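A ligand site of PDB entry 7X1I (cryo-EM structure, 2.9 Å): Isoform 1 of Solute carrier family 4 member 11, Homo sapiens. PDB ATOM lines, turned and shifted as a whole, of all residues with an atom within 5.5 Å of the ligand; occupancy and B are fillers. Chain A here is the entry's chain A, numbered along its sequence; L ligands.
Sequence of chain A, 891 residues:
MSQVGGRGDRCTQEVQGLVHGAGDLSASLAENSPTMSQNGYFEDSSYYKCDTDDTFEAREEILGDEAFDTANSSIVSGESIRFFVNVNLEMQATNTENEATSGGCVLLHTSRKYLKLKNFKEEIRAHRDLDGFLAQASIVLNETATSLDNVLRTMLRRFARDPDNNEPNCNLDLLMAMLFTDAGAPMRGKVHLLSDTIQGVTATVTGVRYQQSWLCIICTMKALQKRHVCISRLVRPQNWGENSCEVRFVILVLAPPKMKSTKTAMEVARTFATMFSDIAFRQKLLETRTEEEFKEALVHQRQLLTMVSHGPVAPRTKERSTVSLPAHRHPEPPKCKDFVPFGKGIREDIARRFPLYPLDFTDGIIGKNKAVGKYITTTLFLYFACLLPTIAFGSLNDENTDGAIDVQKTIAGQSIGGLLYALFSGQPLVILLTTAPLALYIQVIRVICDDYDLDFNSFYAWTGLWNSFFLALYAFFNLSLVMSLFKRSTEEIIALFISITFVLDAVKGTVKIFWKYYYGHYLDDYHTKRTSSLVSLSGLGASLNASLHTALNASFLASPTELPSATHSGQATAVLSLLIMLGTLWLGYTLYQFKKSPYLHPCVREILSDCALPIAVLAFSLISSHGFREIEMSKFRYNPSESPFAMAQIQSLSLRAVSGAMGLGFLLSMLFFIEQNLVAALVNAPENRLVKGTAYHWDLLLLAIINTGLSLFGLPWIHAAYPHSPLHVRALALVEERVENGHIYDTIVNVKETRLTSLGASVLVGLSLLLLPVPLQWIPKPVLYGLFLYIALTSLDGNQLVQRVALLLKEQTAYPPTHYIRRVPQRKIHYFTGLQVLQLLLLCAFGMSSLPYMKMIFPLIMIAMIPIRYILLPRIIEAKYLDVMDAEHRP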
ATOM      1  N   ARG A 125      13.263  17.667 -16.295  1.00  0.00           N
ATOM      2  CA  ARG A 125      13.334  18.536 -15.130  1.00  0.00           C
ATOM      3  C   ARG A 125      12.380  18.115 -14.021  1.00  0.00           C
ATOM      4  O   ARG A 125      12.669  18.366 -12.851  1.00  0.00           O
ATOM      5  CB  ARG A 125      13.063  19.982 -15.528  1.00  0.00           C
ATOM      6  CG  ARG A 125      13.482  20.994 -14.473  1.00  0.00           C
ATOM      7  CD  ARG A 125      14.957  20.862 -14.148  1.00  0.00           C
ATOM      8  NE  ARG A 125      15.207  20.833 -12.709  1.00  0.00           N
ATOM      9  CZ  ARG A 125      16.397  20.666 -12.158  1.00  0.00           C
ATOM     10  NH1 ARG A 125      17.483  20.513 -12.890  1.00  0.00           N
ATOM     11  NH2 ARG A 125      16.492  20.657 -10.830  1.00  0.00           N
ATOM     12  N   ARG A 128      14.340  15.534 -12.217  1.00  0.00           N
ATOM     13  CA  ARG A 128      15.429  16.173 -11.495  1.00  0.00           C
ATOM     14  C   ARG A 128      14.942  16.883 -10.247  1.00  0.00           C
ATOM     15  O   ARG A 128      15.552  16.778  -9.176  1.00  0.00           O
ATOM     16  CB  ARG A 128      16.184  17.134 -12.413  1.00  0.00           C
ATOM     17  CG  ARG A 128      17.304  16.485 -13.209  1.00  0.00           C
ATOM     18  CD  ARG A 128      17.907  17.446 -14.206  1.00  0.00           C
ATOM     19  NE  ARG A 128      19.196  16.978 -14.696  1.00  0.00           N
ATOM     20  CZ  ARG A 128      19.365  16.056 -15.637  1.00  0.00           C
ATOM     21  NH1 ARG A 128      18.330  15.466 -16.212  1.00  0.00           N
ATOM     22  NH2 ARG A 128      20.591  15.699 -16.003  1.00  0.00           N
ATOM     23  N   ASP A 129      13.831  17.618 -10.347  1.00  0.00           N
ATOM     24  CA  ASP A 129      13.274  18.311  -9.197  1.00  0.00           C
ATOM     25  C   ASP A 129      12.811  17.322  -8.130  1.00  0.00           C
ATOM     26  O   ASP A 129      13.046  17.534  -6.929  1.00  0.00           O
ATOM     27  CB  ASP A 129      12.114  19.217  -9.628  1.00  0.00           C
ATOM     28  CG  ASP A 129      12.567  20.348 -10.522  1.00  0.00           C
ATOM     29  OD1 ASP A 129      13.719  20.801 -10.372  1.00  0.00           O
ATOM     30  OD2 ASP A 129      11.763  20.789 -11.368  1.00  0.00           O
ATOM     31  N   ARG A 227      16.912  25.999  -4.368  1.00  0.00           N
ATOM     32  CA  ARG A 227      15.477  25.768  -4.292  1.00  0.00           C
ATOM     33  C   ARG A 227      15.118  24.914  -3.094  1.00  0.00           C
ATOM     34  O   ARG A 227      15.790  23.914  -2.801  1.00  0.00           O
ATOM     35  CB  ARG A 227      14.982  25.109  -5.578  1.00  0.00           C
ATOM     36  CG  ARG A 227      14.867  26.062  -6.756  1.00  0.00           C
ATOM     37  CD  ARG A 227      14.944  25.336  -8.091  1.00  0.00           C
ATOM     38  NE  ARG A 227      16.313  25.068  -8.501  1.00  0.00           N
ATOM     39  CZ  ARG A 227      16.966  23.938  -8.278  1.00  0.00           C
ATOM     40  NH1 ARG A 227      16.393  22.922  -7.645  1.00  0.00           N
ATOM     41  NH2 ARG A 227      18.218  23.816  -8.691  1.00  0.00           N
ATOM     42  N   LYS A 260      17.345  29.384 -14.036  1.00  0.00           N
ATOM     43  CA  LYS A 260      17.019  28.972 -15.398  1.00  0.00           C
ATOM     44  C   LYS A 260      15.517  28.881 -15.586  1.00  0.00           C
ATOM     45  O   LYS A 260      14.770  28.558 -14.658  1.00  0.00           O
ATOM     46  CB  LYS A 260      17.674  27.624 -15.720  1.00  0.00           C
ATOM     47  CG  LYS A 260      19.151  27.542 -15.385  1.00  0.00           C
ATOM     48  CD  LYS A 260      19.710  26.188 -15.733  1.00  0.00           C
ATOM     49  CE  LYS A 260      19.540  25.882 -17.219  1.00  0.00           C
ATOM     50  NZ  LYS A 260      20.023  24.517 -17.552  1.00  0.00           N
ATOM     51  N   THR A 262      13.759  26.759 -16.894  1.00  0.00           N
ATOM     52  CA  THR A 262      13.215  25.426 -16.679  1.00  0.00           C
ATOM     53  C   THR A 262      13.171  25.031 -15.214  1.00  0.00           C
ATOM     54  O   THR A 262      12.488  24.058 -14.879  1.00  0.00           O
ATOM     55  CB  THR A 262      14.023  24.389 -17.463  1.00  0.00           C
ATOM     56  OG1 THR A 262      15.376  24.356 -16.978  1.00  0.00           O
ATOM     57  CG2 THR A 262      14.036  24.716 -18.950  1.00  0.00           C
ATOM     58  N   LYS A 263      13.868  25.745 -14.340  1.00  0.00           N
ATOM     59  CA  LYS A 263      13.938  25.398 -12.926  1.00  0.00           C
ATOM     60  C   LYS A 263      13.581  26.597 -12.054  1.00  0.00           C
ATOM     61  O   LYS A 263      14.122  26.771 -10.947  1.00  0.00           O
ATOM     62  CB  LYS A 263      15.314  24.856 -12.559  1.00  0.00           C
ATOM     63  CG  LYS A 263      16.459  25.789 -12.921  1.00  0.00           C
ATOM     64  CD  LYS A 263      17.787  25.270 -12.382  1.00  0.00           C
ATOM     65  CE  LYS A 263      18.089  23.862 -12.872  1.00  0.00           C
ATOM     66  NZ  LYS A 263      19.369  23.334 -12.332  1.00  0.00           N
ATOM     67  N   LEU A 808      27.206  26.868 -25.263  1.00  0.00           N
ATOM     68  CA  LEU A 808      28.377  26.490 -24.473  1.00  0.00           C
ATOM     69  C   LEU A 808      28.999  27.701 -23.781  1.00  0.00           C
ATOM     70  O   LEU A 808      29.365  27.635 -22.602  1.00  0.00           O
ATOM     71  CB  LEU A 808      29.412  25.799 -25.366  1.00  0.00           C
ATOM     72  CG  LEU A 808      29.025  24.449 -25.967  1.00  0.00           C
ATOM     73  CD1 LEU A 808      30.008  24.060 -27.066  1.00  0.00           C
ATOM     74  CD2 LEU A 808      29.003  23.384 -24.884  1.00  0.00           C
ATOM     75  N   LEU A 809      29.121  28.812 -24.502  1.00  0.00           N
ATOM     76  CA  LEU A 809      29.674  30.042 -23.943  1.00  0.00           C
ATOM     77  C   LEU A 809      28.541  30.949 -23.476  1.00  0.00           C
ATOM     78  O   LEU A 809      28.278  32.028 -24.018  1.00  0.00           O
ATOM     79  CB  LEU A 809      30.561  30.736 -24.981  1.00  0.00           C
ATOM     80  CG  LEU A 809      31.700  29.890 -25.567  1.00  0.00           C
ATOM     81  CD1 LEU A 809      32.444  30.665 -26.636  1.00  0.00           C
ATOM     82  CD2 LEU A 809      32.649  29.437 -24.467  1.00  0.00           C
ATOM     83  N   GLN A 812      24.467  29.649 -17.087  1.00  0.00           N
ATOM     84  CA  GLN A 812      23.357  28.714 -16.939  1.00  0.00           C
ATOM     85  C   GLN A 812      22.009  29.439 -16.858  1.00  0.00           C
ATOM     86  O   GLN A 812      21.026  28.998 -17.467  1.00  0.00           O
ATOM     87  CB  GLN A 812      23.565  27.842 -15.704  1.00  0.00           C
ATOM     88  CG  GLN A 812      24.751  26.884 -15.814  1.00  0.00           C
ATOM     89  CD  GLN A 812      24.521  25.792 -16.828  1.00  0.00           C
ATOM     90  OE1 GLN A 812      23.434  25.212 -16.899  1.00  0.00           O
ATOM     91  NE2 GLN A 812      25.533  25.506 -17.635  1.00  0.00           N
ATOM     92  N   TYR A 815      19.945  30.235 -20.139  1.00  0.00           N
ATOM     93  CA  TYR A 815      19.517  29.196 -21.063  1.00  0.00           C
ATOM     94  C   TYR A 815      18.042  29.352 -21.396  1.00  0.00           C
ATOM     95  O   TYR A 815      17.205  29.339 -20.495  1.00  0.00           O
ATOM     96  CB  TYR A 815      19.775  27.804 -20.467  1.00  0.00           C
ATOM     97  CG  TYR A 815      21.213  27.346 -20.581  1.00  0.00           C
ATOM     98  CD1 TYR A 815      22.243  28.238 -20.856  1.00  0.00           C
ATOM     99  CD2 TYR A 815      21.537  26.005 -20.407  1.00  0.00           C
ATOM    100  CE1 TYR A 815      23.550  27.810 -20.957  1.00  0.00           C
ATOM    101  CE2 TYR A 815      22.850  25.570 -20.505  1.00  0.00           C
ATOM    102  CZ  TYR A 815      23.847  26.478 -20.781  1.00  0.00           C
ATOM    103  OH  TYR A 815      25.155  26.049 -20.883  1.00  0.00           O
ATOM    104  N   GLN A 826      21.322  18.304 -20.329  1.00  0.00           N
ATOM    105  CA  GLN A 826      22.265  19.344 -20.737  1.00  0.00           C
ATOM    106  C   GLN A 826      23.590  18.741 -21.171  1.00  0.00           C
ATOM    107  O   GLN A 826      24.194  19.193 -22.161  1.00  0.00           O
ATOM    108  CB  GLN A 826      22.483  20.325 -19.583  1.00  0.00           C
ATOM    109  CG  GLN A 826      23.478  21.423 -19.895  1.00  0.00           C
ATOM    110  CD  GLN A 826      23.744  22.335 -18.709  1.00  0.00           C
ATOM    111  OE1 GLN A 826      24.484  23.312 -18.812  1.00  0.00           O
ATOM    112  NE2 GLN A 826      23.135  22.022 -17.575  1.00  0.00           N
ATOM    113  N   ARG A 827      24.082  17.725 -20.454  1.00  0.00           N
ATOM    114  CA  ARG A 827      25.333  17.082 -20.832  1.00  0.00           C
ATOM    115  C   ARG A 827      25.221  16.436 -22.207  1.00  0.00           C
ATOM    116  O   ARG A 827      26.158  16.517 -23.013  1.00  0.00           O
ATOM    117  CB  ARG A 827      25.739  16.058 -19.783  1.00  0.00           C
ATOM    118  CG  ARG A 827      26.997  15.285 -20.127  1.00  0.00           C
ATOM    119  CD  ARG A 827      27.379  14.325 -19.012  1.00  0.00           C
ATOM    120  NE  ARG A 827      27.839  15.025 -17.822  1.00  0.00           N
ATOM    121  CZ  ARG A 827      29.108  15.321 -17.572  1.00  0.00           C
ATOM    122  NH1 ARG A 827      30.071  14.988 -18.413  1.00  0.00           N
ATOM    123  NH2 ARG A 827      29.415  15.968 -16.454  1.00  0.00           N
ATOM    124  N   HIS A 830      25.408  19.143 -24.968  1.00  0.00           N
ATOM    125  CA  HIS A 830      26.763  19.587 -25.243  1.00  0.00           C
ATOM    126  C   HIS A 830      27.583  18.518 -25.958  1.00  0.00           C
ATOM    127  O   HIS A 830      28.443  18.851 -26.784  1.00  0.00           O
ATOM    128  CB  HIS A 830      27.446  20.019 -23.949  1.00  0.00           C
ATOM    129  CG  HIS A 830      26.792  21.205 -23.287  1.00  0.00           C
ATOM    130  ND1 HIS A 830      26.002  22.096 -23.975  1.00  0.00           N
ATOM    131  CD2 HIS A 830      26.812  21.622 -22.001  1.00  0.00           C
ATOM    132  CE1 HIS A 830      25.567  23.023 -23.142  1.00  0.00           C
ATOM    133  NE2 HIS A 830      26.037  22.760 -21.935  1.00  0.00           N
ATOM    134  N   TYR A 831      27.340  17.248 -25.641  1.00  0.00           N
ATOM    135  CA  TYR A 831      27.998  16.173 -26.384  1.00  0.00           C
ATOM    136  C   TYR A 831      27.581  16.180 -27.847  1.00  0.00           C
ATOM    137  O   TYR A 831      28.424  16.002 -28.741  1.00  0.00           O
ATOM    138  CB  TYR A 831      27.683  14.818 -25.738  1.00  0.00           C
ATOM    139  CG  TYR A 831      28.391  14.562 -24.436  1.00  0.00           C
ATOM    140  CD1 TYR A 831      29.409  15.402 -23.991  1.00  0.00           C
ATOM    141  CD2 TYR A 831      28.055  13.482 -23.639  1.00  0.00           C
ATOM    142  CE1 TYR A 831      30.058  15.162 -22.794  1.00  0.00           C
ATOM    143  CE2 TYR A 831      28.692  13.233 -22.443  1.00  0.00           C
ATOM    144  CZ  TYR A 831      29.702  14.076 -22.027  1.00  0.00           C
ATOM    145  OH  TYR A 831      30.352  13.846 -20.840  1.00  0.00           O
ATOM    146  N   THR A 833      26.497  18.762 -29.575  1.00  0.00           N
ATOM    147  CA  THR A 833      27.094  19.923 -30.212  1.00  0.00           C
ATOM    148  C   THR A 833      28.551  19.679 -30.582  1.00  0.00           C
ATOM    149  O   THR A 833      28.996  20.045 -31.668  1.00  0.00           O
ATOM    150  CB  THR A 833      26.967  21.146 -29.301  1.00  0.00           C
ATOM    151  OG1 THR A 833      25.584  21.390 -29.006  1.00  0.00           O
ATOM    152  CG2 THR A 833      27.564  22.387 -29.971  1.00  0.00           C
ATOM    153  N   GLY A 834      29.311  19.055 -29.673  1.00  0.00           N
ATOM    154  CA  GLY A 834      30.703  18.748 -29.969  1.00  0.00           C
ATOM    155  C   GLY A 834      30.857  17.782 -31.123  1.00  0.00           C
ATOM    156  O   GLY A 834      31.757  17.919 -31.952  1.00  0.00           O
ATOM    157  N   VAL A 837      30.214  19.635 -34.394  1.00  0.00           N
ATOM    158  CA  VAL A 837      31.393  20.441 -34.752  1.00  0.00           C
ATOM    159  C   VAL A 837      32.479  19.549 -35.343  1.00  0.00           C
ATOM    160  O   VAL A 837      33.161  19.929 -36.298  1.00  0.00           O
ATOM    161  CB  VAL A 837      31.893  21.233 -33.536  1.00  0.00           C
ATOM    162  CG1 VAL A 837      33.213  21.926 -33.845  1.00  0.00           C
ATOM    163  CG2 VAL A 837      30.851  22.243 -33.090  1.00  0.00           C
HETATM  164  O1  LIG L   1      27.140  18.251 -14.041  1.00  0.00           O
HETATM  165  P1  LIG L   1      26.236  17.976 -15.159  1.00  0.00           P
HETATM  166  O2  LIG L   1      26.380  19.071 -16.307  1.00  0.00           O
HETATM  167  O3  LIG L   1      26.408  16.617 -15.815  1.00  0.00           O
HETATM  168  O4  LIG L   1      22.652  19.619 -15.859  1.00  0.00           O
HETATM  169  O5  LIG L   1      24.725  18.101 -14.726  1.00  0.00           O
HETATM  170  C1  LIG L   1      23.975  19.036 -13.927  1.00  0.00           C
HETATM  171  C2  LIG L   1      22.576  19.188 -14.506  1.00  0.00           C
HETATM  172  C3  LIG L   1      23.909  18.519 -12.496  1.00  0.00           C
HETATM  173  O6  LIG L   1      25.213  18.282 -11.998  1.00  0.00           O
HETATM  174  C4  LIG L   1      23.194  19.536 -11.631  1.00  0.00           C
HETATM  175  O7  LIG L   1      23.093  19.060 -10.296  1.00  0.00           O
HETATM  176  C5  LIG L   1      21.812  19.828 -12.191  1.00  0.00           C
HETATM  177  O8  LIG L   1      21.236  20.927 -11.449  1.00  0.00           O
HETATM  178  P2  LIG L   1      20.375  20.844 -10.095  1.00  0.00           P
HETATM  179  O9  LIG L   1      20.934  21.777  -9.097  1.00  0.00           O
HETATM  180  O10 LIG L   1      20.413  19.379  -9.653  1.00  0.00           O
HETATM  181  O11 LIG L   1      18.948  21.168 -10.494  1.00  0.00           O
HETATM  182  C6  LIG L   1      21.848  20.223 -13.667  1.00  0.00           C
HETATM  183  O12 LIG L   1      20.492  20.333 -14.138  1.00  0.00           O
HETATM  184  P3  LIG L   1      20.024  21.254 -15.367  1.00  0.00           P
HETATM  185  O13 LIG L   1      20.682  20.812 -16.611  1.00  0.00           O
HETATM  186  O14 LIG L   1      20.392  22.685 -14.979  1.00  0.00           O
HETATM  187  O15 LIG L   1      18.511  21.150 -15.422  1.00  0.00           O
HETATM  188  C7  LIG L   1      27.636  19.681 -16.670  1.00  0.00           C
HETATM  189  C8  LIG L   1      27.543  20.247 -18.066  1.00  0.00           C
HETATM  190  C9  LIG L   1      27.158  21.696 -18.028  1.00  0.00           C
HETATM  191  O16 LIG L   1      28.871  20.166 -18.652  1.00  0.00           O
HETATM  192  C10 LIG L   1      29.083  19.237 -19.590  1.00  0.00           C
HETATM  193  O17 LIG L   1      28.944  18.060 -19.421  1.00  0.00           O
HETATM  194  O18 LIG L   1      28.109  22.421 -18.847  1.00  0.00           O
HETATM  195  C11 LIG L   1      28.632  23.528 -18.332  1.00  0.00           C
HETATM  196  O19 LIG L   1      28.311  23.983 -17.257  1.00  0.00           O
HETATM  197  C12 LIG L   1      29.530  19.863 -20.882  1.00  0.00           C
HETATM  198  C13 LIG L   1      30.369  18.929 -21.749  1.00  0.00           C
HETATM  199  C14 LIG L   1      30.982  19.625 -22.960  1.00  0.00           C
HETATM  200  C15 LIG L   1      31.398  18.665 -24.057  1.00  0.00           C
HETATM  201  C16 LIG L   1      32.376  19.240 -25.063  1.00  0.00           C
HETATM  202  C17 LIG L   1      31.788  20.265 -26.008  1.00  0.00           C
HETATM  203  C18 LIG L   1      32.763  20.702 -27.098  1.00  0.00           C
HETATM  204  C19 LIG L   1      32.179  21.663 -28.084  1.00  0.00           C
HETATM  205  C20 LIG L   1      32.772  22.117 -29.173  1.00  0.00           C
HETATM  206  C21 LIG L   1      33.201  23.522 -29.423  1.00  0.00           C
HETATM  207  C22 LIG L   1      29.655  24.139 -19.246  1.00  0.00           C
HETATM  208  C23 LIG L   1      29.602  23.572 -20.663  1.00  0.00           C
HETATM  209  C24 LIG L   1      30.609  24.213 -21.600  1.00  0.00           C
HETATM  210  C25 LIG L   1      32.053  23.930 -21.247  1.00  0.00           C
HETATM  211  C26 LIG L   1      33.061  24.520 -22.223  1.00  0.00           C
HETATM  212  C27 LIG L   1      32.955  23.971 -23.633  1.00  0.00           C
HETATM  213  C28 LIG L   1      34.072  24.443 -24.571  1.00  0.00           C
HETATM  214  C29 LIG L   1      34.110  25.928 -24.732  1.00  0.00           C
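OD1 of Asp 129 is in salt-bridge range of NE of Arg 125, at 2.8 Å. The side-chain amide oxygen (OE1) of Gln 826 lies within hydrogen-bond range of the side-chain amide nitrogen (NE2) of Gln 812 (2.7 Å). The side-chain amide oxygen (OE1) of Gln 826 lies close to the side-chain hydroxyl (OH) of Tyr 815, 3.5 Å away. The side-chain hydroxyl (OH) of Tyr 831 is in hydrogen-bond range of the guanidinium group (NH1) of Arg 827 (2.7 Å). NE2 of Gln 812 lies within hydrogen-bond range of OH of Tyr 815 (3.3 Å).
Merely in contact with the ligand: Leu 808 (3.4 Å), His 830 (3.4 Å), Arg 128 (3.6 Å), Gly 834 (3.8 Å), Leu 809 (3.8 Å) and Tyr 831 (3.8 Å). Hydrophobic or aromatic side chains within 4 Å of the ligand: Leu 808, Leu 809, His 830 and Tyr 831. Along chain A the residues within 4 Å of the ligand span positions 125 to 834. The nearest printed residue that does not touch the ligand is Val 837 (4.4 Å).
O11 of the ligand lies within salt-bridge range of NH2 of Arg 125 (2.5 Å). NZ of Lys 263 is in salt-bridge range of O11 of the ligand (2.9 Å). NE2 of Gln 826 sits at hydrogen-bond distance from O13 of the ligand (2.9 Å). O3 of the ligand lies within salt-bridge range of NE of Arg 827. O14 of the ligand lies within salt-bridge range of NZ of Lys 260 (3.2 Å). The side-chain amide nitrogen (NE2) of Gln 812 lies within hydrogen-bond range of an oxygen (O19) of the ligand, at 3.2 Å. The guanidinium group of Arg 227 is in salt-bridge range of an oxygen (O11) of the ligand, at 3.3 Å.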
